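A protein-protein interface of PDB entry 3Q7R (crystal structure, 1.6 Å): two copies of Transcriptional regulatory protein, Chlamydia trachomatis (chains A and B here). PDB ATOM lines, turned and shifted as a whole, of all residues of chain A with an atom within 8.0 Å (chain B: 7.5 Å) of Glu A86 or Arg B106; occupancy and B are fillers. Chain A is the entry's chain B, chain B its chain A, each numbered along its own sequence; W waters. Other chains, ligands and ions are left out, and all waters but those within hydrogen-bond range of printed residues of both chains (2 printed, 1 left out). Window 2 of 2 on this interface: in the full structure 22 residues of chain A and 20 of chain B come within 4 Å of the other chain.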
ATOM      1  N   TYR A  58      14.508   0.220 -15.174  1.00  0.00           N
ATOM      2  CA  TYR A  58      14.497   1.239 -16.229  1.00  0.00           C
ATOM      3  C   TYR A  58      15.815   1.284 -17.020  1.00  0.00           C
ATOM      4  O   TYR A  58      15.812   1.469 -18.233  1.00  0.00           O
ATOM      5  CB  TYR A  58      14.210   2.627 -15.650  1.00  0.00           C
ATOM      6  CG  TYR A  58      14.083   3.687 -16.728  1.00  0.00           C
ATOM      7  CD1 TYR A  58      12.958   3.739 -17.534  1.00  0.00           C
ATOM      8  CD2 TYR A  58      15.090   4.619 -16.951  1.00  0.00           C
ATOM      9  CE1 TYR A  58      12.809   4.699 -18.520  1.00  0.00           C
ATOM     10  CE2 TYR A  58      14.956   5.588 -17.941  1.00  0.00           C
ATOM     11  CZ  TYR A  58      13.811   5.617 -18.723  1.00  0.00           C
ATOM     12  OH  TYR A  58      13.631   6.563 -19.698  1.00  0.00           O
ATOM     13  N   PHE A  82      14.954   7.051  -9.613  1.00  0.00           N
ATOM     14  CA  PHE A  82      14.687   8.463  -9.347  1.00  0.00           C
ATOM     15  C   PHE A  82      13.377   8.890  -9.979  1.00  0.00           C
ATOM     16  O   PHE A  82      12.966   8.344 -11.005  1.00  0.00           O
ATOM     17  CB  PHE A  82      15.773   9.280 -10.054  1.00  0.00           C
ATOM     18  CG  PHE A  82      15.914   8.921 -11.517  1.00  0.00           C
ATOM     19  CD1 PHE A  82      14.991   9.382 -12.450  1.00  0.00           C
ATOM     20  CD2 PHE A  82      16.931   8.087 -11.954  1.00  0.00           C
ATOM     21  CE1 PHE A  82      15.087   9.036 -13.789  1.00  0.00           C
ATOM     22  CE2 PHE A  82      17.033   7.734 -13.298  1.00  0.00           C
ATOM     23  CZ  PHE A  82      16.109   8.217 -14.217  1.00  0.00           C
ATOM     24  N   PHE A  83      12.783   9.939  -9.427  1.00  0.00           N
ATOM     25  CA  PHE A  83      11.680  10.614 -10.090  1.00  0.00           C
ATOM     26  C   PHE A  83      12.125  11.614 -11.155  1.00  0.00           C
ATOM     27  O   PHE A  83      12.981  12.469 -10.924  1.00  0.00           O
ATOM     28  CB  PHE A  83      10.829  11.381  -9.096  1.00  0.00           C
ATOM     29  CG  PHE A  83       9.749  12.175  -9.754  1.00  0.00           C
ATOM     30  CD1 PHE A  83       8.666  11.524 -10.332  1.00  0.00           C
ATOM     31  CD2 PHE A  83       9.825  13.556  -9.826  1.00  0.00           C
ATOM     32  CE1 PHE A  83       7.664  12.248 -10.952  1.00  0.00           C
ATOM     33  CE2 PHE A  83       8.828  14.284 -10.458  1.00  0.00           C
ATOM     34  CZ  PHE A  83       7.739  13.615 -11.014  1.00  0.00           C
ATOM     35  N   ASP A  84      11.494  11.522 -12.309  1.00  0.00           N
ATOM     36  CA  ASP A  84      11.640  12.510 -13.375  1.00  0.00           C
ATOM     37  C   ASP A  84      10.301  12.586 -14.116  1.00  0.00           C
ATOM     38  O   ASP A  84       9.801  11.568 -14.586  1.00  0.00           O
ATOM     39  CB  ASP A  84      12.751  12.121 -14.345  1.00  0.00           C
ATOM     40  CG  ASP A  84      12.877  13.116 -15.474  1.00  0.00           C
ATOM     41  OD1 ASP A  84      13.394  14.221 -15.213  1.00  0.00           O
ATOM     42  OD2 ASP A  84      12.430  12.817 -16.599  1.00  0.00           O
ATOM     43  N   GLU A  85       9.700  13.772 -14.215  1.00  0.00           N
ATOM     44  CA  GLU A  85       8.365  13.845 -14.799  1.00  0.00           C
ATOM     45  C   GLU A  85       8.309  13.327 -16.243  1.00  0.00           C
ATOM     46  O   GLU A  85       7.414  12.558 -16.586  1.00  0.00           O
ATOM     47  CB  GLU A  85       7.756  15.250 -14.698  1.00  0.00           C
ATOM     48  CG  GLU A  85       6.342  15.316 -15.279  1.00  0.00           C
ATOM     49  CD  GLU A  85       5.803  16.725 -15.400  1.00  0.00           C
ATOM     50  OE1 GLU A  85       6.604  17.698 -15.469  1.00  0.00           O
ATOM     51  OE2 GLU A  85       4.570  16.859 -15.482  1.00  0.00           O
ATOM     52  N   GLU A  86       9.230  13.735 -17.108  1.00  0.00           N
ATOM     53  CA  GLU A  86       9.171  13.248 -18.477  1.00  0.00           C
ATOM     54  C   GLU A  86       9.290  11.717 -18.553  1.00  0.00           C
ATOM     55  O   GLU A  86       8.610  11.059 -19.356  1.00  0.00           O
ATOM     56  CB  GLU A  86      10.270  13.896 -19.335  1.00  0.00           C
ATOM     57  CG  GLU A  86      10.117  15.394 -19.494  1.00  0.00           C
ATOM     58  CD  GLU A  86       8.866  15.780 -20.264  1.00  0.00           C
ATOM     59  OE1 GLU A  86       8.373  14.947 -21.054  1.00  0.00           O
ATOM     60  OE2 GLU A  86       8.380  16.920 -20.080  1.00  0.00           O
ATOM     61  N   THR A  87      10.190  11.152 -17.758  1.00  0.00           N
ATOM     62  CA  THR A  87      10.377   9.706 -17.753  1.00  0.00           C
ATOM     63  C   THR A  87       9.082   9.014 -17.349  1.00  0.00           C
ATOM     64  O   THR A  87       8.682   8.037 -17.968  1.00  0.00           O
ATOM     65  CB  THR A  87      11.500   9.314 -16.788  1.00  0.00           C
ATOM     66  OG1 THR A  87      12.713   9.958 -17.216  1.00  0.00           O
ATOM     67  CG2 THR A  87      11.727   7.817 -16.788  1.00  0.00           C
ATOM     68  N   SER A  88       8.436   9.524 -16.296  1.00  0.00           N
ATOM     69  CA  SER A  88       7.187   8.936 -15.803  1.00  0.00           C
ATOM     70  C   SER A  88       6.098   8.992 -16.867  1.00  0.00           C
ATOM     71  O   SER A  88       5.398   8.003 -17.112  1.00  0.00           O
ATOM     72  CB  SER A  88       6.676   9.664 -14.559  1.00  0.00           C
ATOM     73  OG  SER A  88       7.507   9.428 -13.445  1.00  0.00           O
ATOM     74  N   VAL A  89       5.907  10.169 -17.461  1.00  0.00           N
ATOM     75  CA  VAL A  89       4.876  10.316 -18.497  1.00  0.00           C
ATOM     76  C   VAL A  89       5.163   9.381 -19.673  1.00  0.00           C
ATOM     77  O   VAL A  89       4.270   8.697 -20.153  1.00  0.00           O
ATOM     78  CB  VAL A  89       4.765  11.756 -18.996  1.00  0.00           C
ATOM     79  CG1 VAL A  89       3.824  11.832 -20.196  1.00  0.00           C
ATOM     80  CG2 VAL A  89       4.258  12.656 -17.895  1.00  0.00           C
ATOM     81  N   ASP A  90       6.415   9.341 -20.125  1.00  0.00           N
ATOM     82  CA  ASP A  90       6.791   8.477 -21.234  1.00  0.00           C
ATOM     83  C   ASP A  90       6.474   7.017 -20.939  1.00  0.00           C
ATOM     84  O   ASP A  90       5.906   6.317 -21.750  1.00  0.00           O
ATOM     85  CB  ASP A  90       8.294   8.638 -21.533  1.00  0.00           C
ATOM     86  CG  ASP A  90       8.758   7.743 -22.679  1.00  0.00           C
ATOM     87  OD1 ASP A  90       8.206   7.866 -23.793  1.00  0.00           O
ATOM     88  OD2 ASP A  90       9.642   6.904 -22.443  1.00  0.00           O
ATOM     89  N   LEU A  91       6.790   6.568 -19.734  1.00  0.00           N
ATOM     90  CA  LEU A  91       6.593   5.158 -19.392  1.00  0.00           C
ATOM     91  C   LEU A  91       5.116   4.823 -19.375  1.00  0.00           C
ATOM     92  O   LEU A  91       4.700   3.807 -19.917  1.00  0.00           O
ATOM     93  CB  LEU A  91       7.155   4.854 -17.988  1.00  0.00           C
ATOM     94  CG  LEU A  91       8.687   4.655 -17.961  1.00  0.00           C
ATOM     95  CD1 LEU A  91       9.147   4.486 -16.493  1.00  0.00           C
ATOM     96  CD2 LEU A  91       9.113   3.456 -18.838  1.00  0.00           C
ATOM     97  N   LEU A  92       4.322   5.674 -18.732  1.00  0.00           N
ATOM     98  CA  LEU A  92       2.881   5.405 -18.654  1.00  0.00           C
ATOM     99  C   LEU A  92       2.249   5.388 -20.059  1.00  0.00           C
ATOM    100  O   LEU A  92       1.421   4.533 -20.369  1.00  0.00           O
ATOM    101  CB  LEU A  92       2.158   6.451 -17.793  1.00  0.00           C
ATOM    102  CG  LEU A  92       2.588   6.420 -16.312  1.00  0.00           C
ATOM    103  CD1 LEU A  92       2.207   7.731 -15.587  1.00  0.00           C
ATOM    104  CD2 LEU A  92       2.079   5.183 -15.591  1.00  0.00           C
ATOM    105  N   ASP A  93       2.630   6.346 -20.887  1.00  0.00           N
ATOM    106  CA  ASP A  93       2.100   6.414 -22.261  1.00  0.00           C
ATOM    107  C   ASP A  93       2.486   5.192 -23.080  1.00  0.00           C
ATOM    108  O   ASP A  93       1.748   4.787 -23.961  1.00  0.00           O
ATOM    109  CB  ASP A  93       2.565   7.688 -22.952  1.00  0.00           C
ATOM    110  CG  ASP A  93       1.831   8.932 -22.440  1.00  0.00           C
ATOM    111  OD1 ASP A  93       0.838   8.779 -21.680  1.00  0.00           O
ATOM    112  OD2 ASP A  93       2.264  10.044 -22.799  1.00  0.00           O
ATOM    113  N   LEU B  24      -4.990  20.341  -9.258  1.00  0.00           N
ATOM    114  CA  LEU B  24      -4.695  19.065  -9.909  1.00  0.00           C
ATOM    115  C   LEU B  24      -5.934  18.580 -10.707  1.00  0.00           C
ATOM    116  O   LEU B  24      -5.816  18.117 -11.832  1.00  0.00           O
ATOM    117  CB  LEU B  24      -4.269  17.994  -8.897  1.00  0.00           C
ATOM    118  CG  LEU B  24      -4.026  16.587  -9.458  1.00  0.00           C
ATOM    119  CD1 LEU B  24      -2.803  16.540 -10.414  1.00  0.00           C
ATOM    120  CD2 LEU B  24      -3.839  15.606  -8.273  1.00  0.00           C
ATOM    121  N   GLN B  27      -6.673  20.903 -13.861  1.00  0.00           N
ATOM    122  CA  GLN B  27      -5.604  20.795 -14.845  1.00  0.00           C
ATOM    123  C   GLN B  27      -5.565  19.417 -15.492  1.00  0.00           C
ATOM    124  O   GLN B  27      -5.284  19.307 -16.698  1.00  0.00           O
ATOM    125  CB  GLN B  27      -4.257  21.145 -14.227  1.00  0.00           C
ATOM    126  CG  GLN B  27      -4.238  22.635 -13.892  1.00  0.00           C
ATOM    127  CD  GLN B  27      -2.957  23.076 -13.265  1.00  0.00           C
ATOM    128  OE1 GLN B  27      -1.897  22.545 -13.571  1.00  0.00           O
ATOM    129  NE2 GLN B  27      -3.040  24.065 -12.382  1.00  0.00           N
ATOM    130  N   THR B  28      -5.852  18.370 -14.706  1.00  0.00           N
ATOM    131  CA  THR B  28      -5.882  17.038 -15.268  1.00  0.00           C
ATOM    132  C   THR B  28      -7.079  16.891 -16.190  1.00  0.00           C
ATOM    133  O   THR B  28      -6.973  16.325 -17.257  1.00  0.00           O
ATOM    134  CB  THR B  28      -5.924  15.973 -14.159  1.00  0.00           C
ATOM    135  OG1 THR B  28      -4.742  16.082 -13.362  1.00  0.00           O
ATOM    136  CG2 THR B  28      -5.955  14.574 -14.796  1.00  0.00           C
ATOM    137  N   LEU B  31      -6.630  18.030 -19.710  1.00  0.00           N
ATOM    138  CA  LEU B  31      -5.742  17.226 -20.553  1.00  0.00           C
ATOM    139  C   LEU B  31      -6.396  15.963 -21.079  1.00  0.00           C
ATOM    140  O   LEU B  31      -5.861  15.337 -22.002  1.00  0.00           O
ATOM    141  CB  LEU B  31      -4.473  16.849 -19.780  1.00  0.00           C
ATOM    142  CG  LEU B  31      -3.620  18.042 -19.316  1.00  0.00           C
ATOM    143  CD1 LEU B  31      -2.470  17.600 -18.425  1.00  0.00           C
ATOM    144  CD2 LEU B  31      -3.085  18.822 -20.536  1.00  0.00           C
ATOM    145  N   ILE B 103       3.064  14.354  -8.191  1.00  0.00           N
ATOM    146  CA  ILE B 103       2.053  13.904  -9.157  1.00  0.00           C
ATOM    147  C   ILE B 103       1.556  15.164  -9.844  1.00  0.00           C
ATOM    148  O   ILE B 103       0.855  15.979  -9.233  1.00  0.00           O
ATOM    149  CB  ILE B 103       0.851  13.250  -8.514  1.00  0.00           C
ATOM    150  CG1 ILE B 103       1.222  11.884  -7.924  1.00  0.00           C
ATOM    151  CG2 ILE B 103      -0.227  12.971  -9.573  1.00  0.00           C
ATOM    152  CD1 ILE B 103       0.217  11.387  -6.880  1.00  0.00           C
ATOM    153  N   THR B 104       1.923  15.312 -11.112  1.00  0.00           N
ATOM    154  CA  THR B 104       1.548  16.469 -11.929  1.00  0.00           C
ATOM    155  C   THR B 104       0.334  16.100 -12.770  1.00  0.00           C
ATOM    156  O   THR B 104      -0.015  14.913 -12.877  1.00  0.00           O
ATOM    157  CB  THR B 104       2.665  16.834 -12.905  1.00  0.00           C
ATOM    158  OG1 THR B 104       2.887  15.740 -13.815  1.00  0.00           O
ATOM    159  CG2 THR B 104       3.985  17.210 -12.164  1.00  0.00           C
ATOM    160  N   PRO B 105      -0.363  17.115 -13.316  1.00  0.00           N
ATOM    161  CA  PRO B 105      -1.483  16.764 -14.194  1.00  0.00           C
ATOM    162  C   PRO B 105      -1.098  15.868 -15.363  1.00  0.00           C
ATOM    163  O   PRO B 105      -1.913  15.004 -15.712  1.00  0.00           O
ATOM    164  CB  PRO B 105      -1.991  18.122 -14.687  1.00  0.00           C
ATOM    165  CG  PRO B 105      -1.660  19.057 -13.537  1.00  0.00           C
ATOM    166  CD  PRO B 105      -0.321  18.556 -13.001  1.00  0.00           C
ATOM    167  N   ARG B 106       0.075  16.050 -15.974  1.00  0.00           N
ATOM    168  CA  ARG B 106       0.468  15.172 -17.075  1.00  0.00           C
ATOM    169  C   ARG B 106       0.611  13.707 -16.591  1.00  0.00           C
ATOM    170  O   ARG B 106       0.227  12.790 -17.285  1.00  0.00           O
ATOM    171  CB  ARG B 106       1.783  15.676 -17.714  1.00  0.00           C
ATOM    172  CG  ARG B 106       1.570  16.898 -18.586  1.00  0.00           C
ATOM    173  CD  ARG B 106       2.898  17.468 -19.070  1.00  0.00           C
ATOM    174  NE  ARG B 106       3.508  16.581 -20.058  1.00  0.00           N
ATOM    175  CZ  ARG B 106       4.810  16.324 -20.138  1.00  0.00           C
ATOM    176  NH1 ARG B 106       5.654  16.891 -19.291  1.00  0.00           N
ATOM    177  NH2 ARG B 106       5.257  15.501 -21.065  1.00  0.00           N
ATOM    178  N   ILE B 107       1.153  13.498 -15.405  1.00  0.00           N
ATOM    179  CA  ILE B 107       1.285  12.128 -14.894  1.00  0.00           C
ATOM    180  C   ILE B 107      -0.073  11.559 -14.600  1.00  0.00           C
ATOM    181  O   ILE B 107      -0.336  10.408 -14.928  1.00  0.00           O
ATOM    182  CB  ILE B 107       2.138  12.129 -13.667  1.00  0.00           C
ATOM    183  CG1 ILE B 107       3.577  12.451 -14.094  1.00  0.00           C
ATOM    184  CG2 ILE B 107       2.044  10.774 -12.914  1.00  0.00           C
ATOM    185  CD1 ILE B 107       4.543  12.615 -12.953  1.00  0.00           C
ATOM    186  N   LEU B 108      -0.923  12.326 -13.914  1.00  0.00           N
ATOM    187  CA  LEU B 108      -2.210  11.751 -13.525  1.00  0.00           C
ATOM    188  C   LEU B 108      -3.048  11.434 -14.782  1.00  0.00           C
ATOM    189  O   LEU B 108      -3.717  10.381 -14.852  1.00  0.00           O
ATOM    190  CB  LEU B 108      -2.951  12.699 -12.572  1.00  0.00           C
ATOM    191  CG  LEU B 108      -4.303  12.174 -12.120  1.00  0.00           C
ATOM    192  CD1 LEU B 108      -4.198  10.798 -11.345  1.00  0.00           C
ATOM    193  CD2 LEU B 108      -5.002  13.188 -11.224  1.00  0.00           C
ATOM    194  N   LYS B 109      -3.017  12.326 -15.791  1.00  0.00           N
ATOM    195  CA  LYS B 109      -3.719  12.037 -17.027  1.00  0.00           C
ATOM    196  C   LYS B 109      -3.238  10.731 -17.654  1.00  0.00           C
ATOM    197  O   LYS B 109      -4.048   9.908 -18.100  1.00  0.00           O
ATOM    198  CB  LYS B 109      -3.485  13.197 -18.026  1.00  0.00           C
ATOM    199  CG  LYS B 109      -4.131  12.974 -19.416  1.00  0.00           C
ATOM    200  CD  LYS B 109      -3.113  12.408 -20.407  1.00  0.00           C
ATOM    201  CE  LYS B 109      -3.551  12.618 -21.874  1.00  0.00           C
ATOM    202  NZ  LYS B 109      -2.687  11.826 -22.795  1.00  0.00           N
ATOM    203  N   SER B 110      -1.924  10.528 -17.689  1.00  0.00           N
ATOM    204  CA  SER B 110      -1.372   9.325 -18.299  1.00  0.00           C
ATOM    205  C   SER B 110      -1.712   8.083 -17.494  1.00  0.00           C
ATOM    206  O   SER B 110      -1.951   7.012 -18.058  1.00  0.00           O
ATOM    207  CB  SER B 110       0.149   9.450 -18.512  1.00  0.00           C
ATOM    208  OG  SER B 110       0.425  10.443 -19.512  1.00  0.00           O
ATOM    209  N   ALA B 111      -1.712   8.230 -16.171  1.00  0.00           N
ATOM    210  CA  ALA B 111      -1.992   7.100 -15.313  1.00  0.00           C
ATOM    211  C   ALA B 111      -3.450   6.676 -15.424  1.00  0.00           C
ATOM    212  O   ALA B 111      -3.738   5.489 -15.431  1.00  0.00           O
ATOM    213  CB  ALA B 111      -1.666   7.459 -13.855  1.00  0.00           C
ATOM    214  N   ILE B 112      -4.366   7.643 -15.381  1.00  0.00           N
ATOM    215  CA  ILE B 112      -5.785   7.345 -15.544  1.00  0.00           C
ATOM    216  C   ILE B 112      -6.013   6.653 -16.882  1.00  0.00           C
ATOM    217  O   ILE B 112      -6.727   5.650 -16.976  1.00  0.00           O
ATOM    218  CB  ILE B 112      -6.583   8.678 -15.481  1.00  0.00           C
ATOM    219  CG1 ILE B 112      -6.635   9.201 -14.048  1.00  0.00           C
ATOM    220  CG2 ILE B 112      -7.985   8.525 -16.090  1.00  0.00           C
ATOM    221  CD1 ILE B 112      -7.148  10.694 -13.998  1.00  0.00           C
HETATM  222  O   HOH W   1       0.731  12.179 -22.430  1.00  0.00           O
HETATM  223  O   HOH W   2       1.641  18.480 -15.914  1.00  0.00           O
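OE2 of Glu A85 sits at hydrogen-bond distance from OG1 of Thr B104 (2.6 Å).
The guanidinium group (NH1) of Arg B106 lies within salt-bridge range of the side-chain carboxylate (OE2) of Glu A85 (3.96 Å).
The guanidinium group (NH1) of Arg B106 lies within salt-bridge range of the side-chain carboxylate (OE2) of Glu A86 (2.8 Å).
OD1 of Asp A93 is in hydrogen-bond range of OG of Ser B110 (2.8 Å).
OG1 of Thr B104 lies within hydrogen-bond range of N of Ile B107 (3.2 Å).
O of Arg B106 sits at hydrogen-bond distance from OG of Ser B110 (3.2 Å).
OD2 of Asp A84 sits at hydrogen-bond distance from N of Glu A86 (3.4 Å).
OG of Ser A88 lies within hydrogen-bond range of O of Asp A84 (3.3 Å).
Among the printed residues, pairs that only touch across the chains: Leu A92 with Ser B110 (3.7 Å), Phe A83 with Ile B107 (3.7 Å), Val A89 with Ser B110 (3.7 Å), Leu A92 with Ile B107 (3.8 Å), Val A89 with Ile B107 (3.9 Å), Val A89 with Arg B106 (3.9 Å), Ser A88 with Ile B107 (3.98 Å), Glu A85 with Ile B107 (3.99 Å) and Leu A92 with Ala B111 (3.99 Å).
Water W1 lies within hydrogen-bond range of OD2 of Asp A93 (2.7 Å), OG of Ser B110 (3.4 Å) and NZ of Lys B109 (3.5 Å).
Water W2 bridges N of Arg B106 and OE2 of Glu A85.
Printed residues of chain B within 4 Å of Glu A85: Thr B104 (2.6 Å), Arg B106 (3.8 Å) and Ile B107 (3.99 Å).
Of chain B, only Arg B106 comes within 4 Å of Glu A86.
Printed residues of chain B within 4 Å of Val A89: Arg B106, Ile B107 and Ser B110.
Of the printed residues of chain B, Asp A93 touches Ser B110 (2.8 Å).
Of the printed residues of chain A, Thr B104 touches Glu A85 (2.6 Å).
Printed residues of chain A within 4 Å of Ala B111: Leu A92 (3.99 Å).
The nearest residue of chain B that does not touch Glu A86 is Ile B107 (6.4 Å).
No position is printed for both chains.
Of the 14 printed residues of chain B, 5 touch a printed residue of chain A.
Printed residues of chain B that touch a printed residue of chain A: Thr B104, Arg B106, Ile B107, Ser B110 and Ala B111.
Hydrophobic or aromatic side chains of chain B that line the printed part of chain A: Ile B107.
Of the 13 printed residues of chain A, 7 touch a printed residue of chain B.
Printed residues of chain A that touch a printed residue of chain B: Phe A83, Glu A85, Glu A86, Ser A88, Val A89, Leu A92 and Asp A93.
Hydrophobic or aromatic side chains of chain A within 4 Å of the printed part of chain B: Phe A83, Val A89 and Leu A92.
Among the printed residues, Asp or Glu carboxylates within 4 Å of a Lys or Arg side-chain nitrogen of the other chain: Glu A85 with Arg B106 (3.96 Å) and Glu A86 with Arg B106 (2.8 Å).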
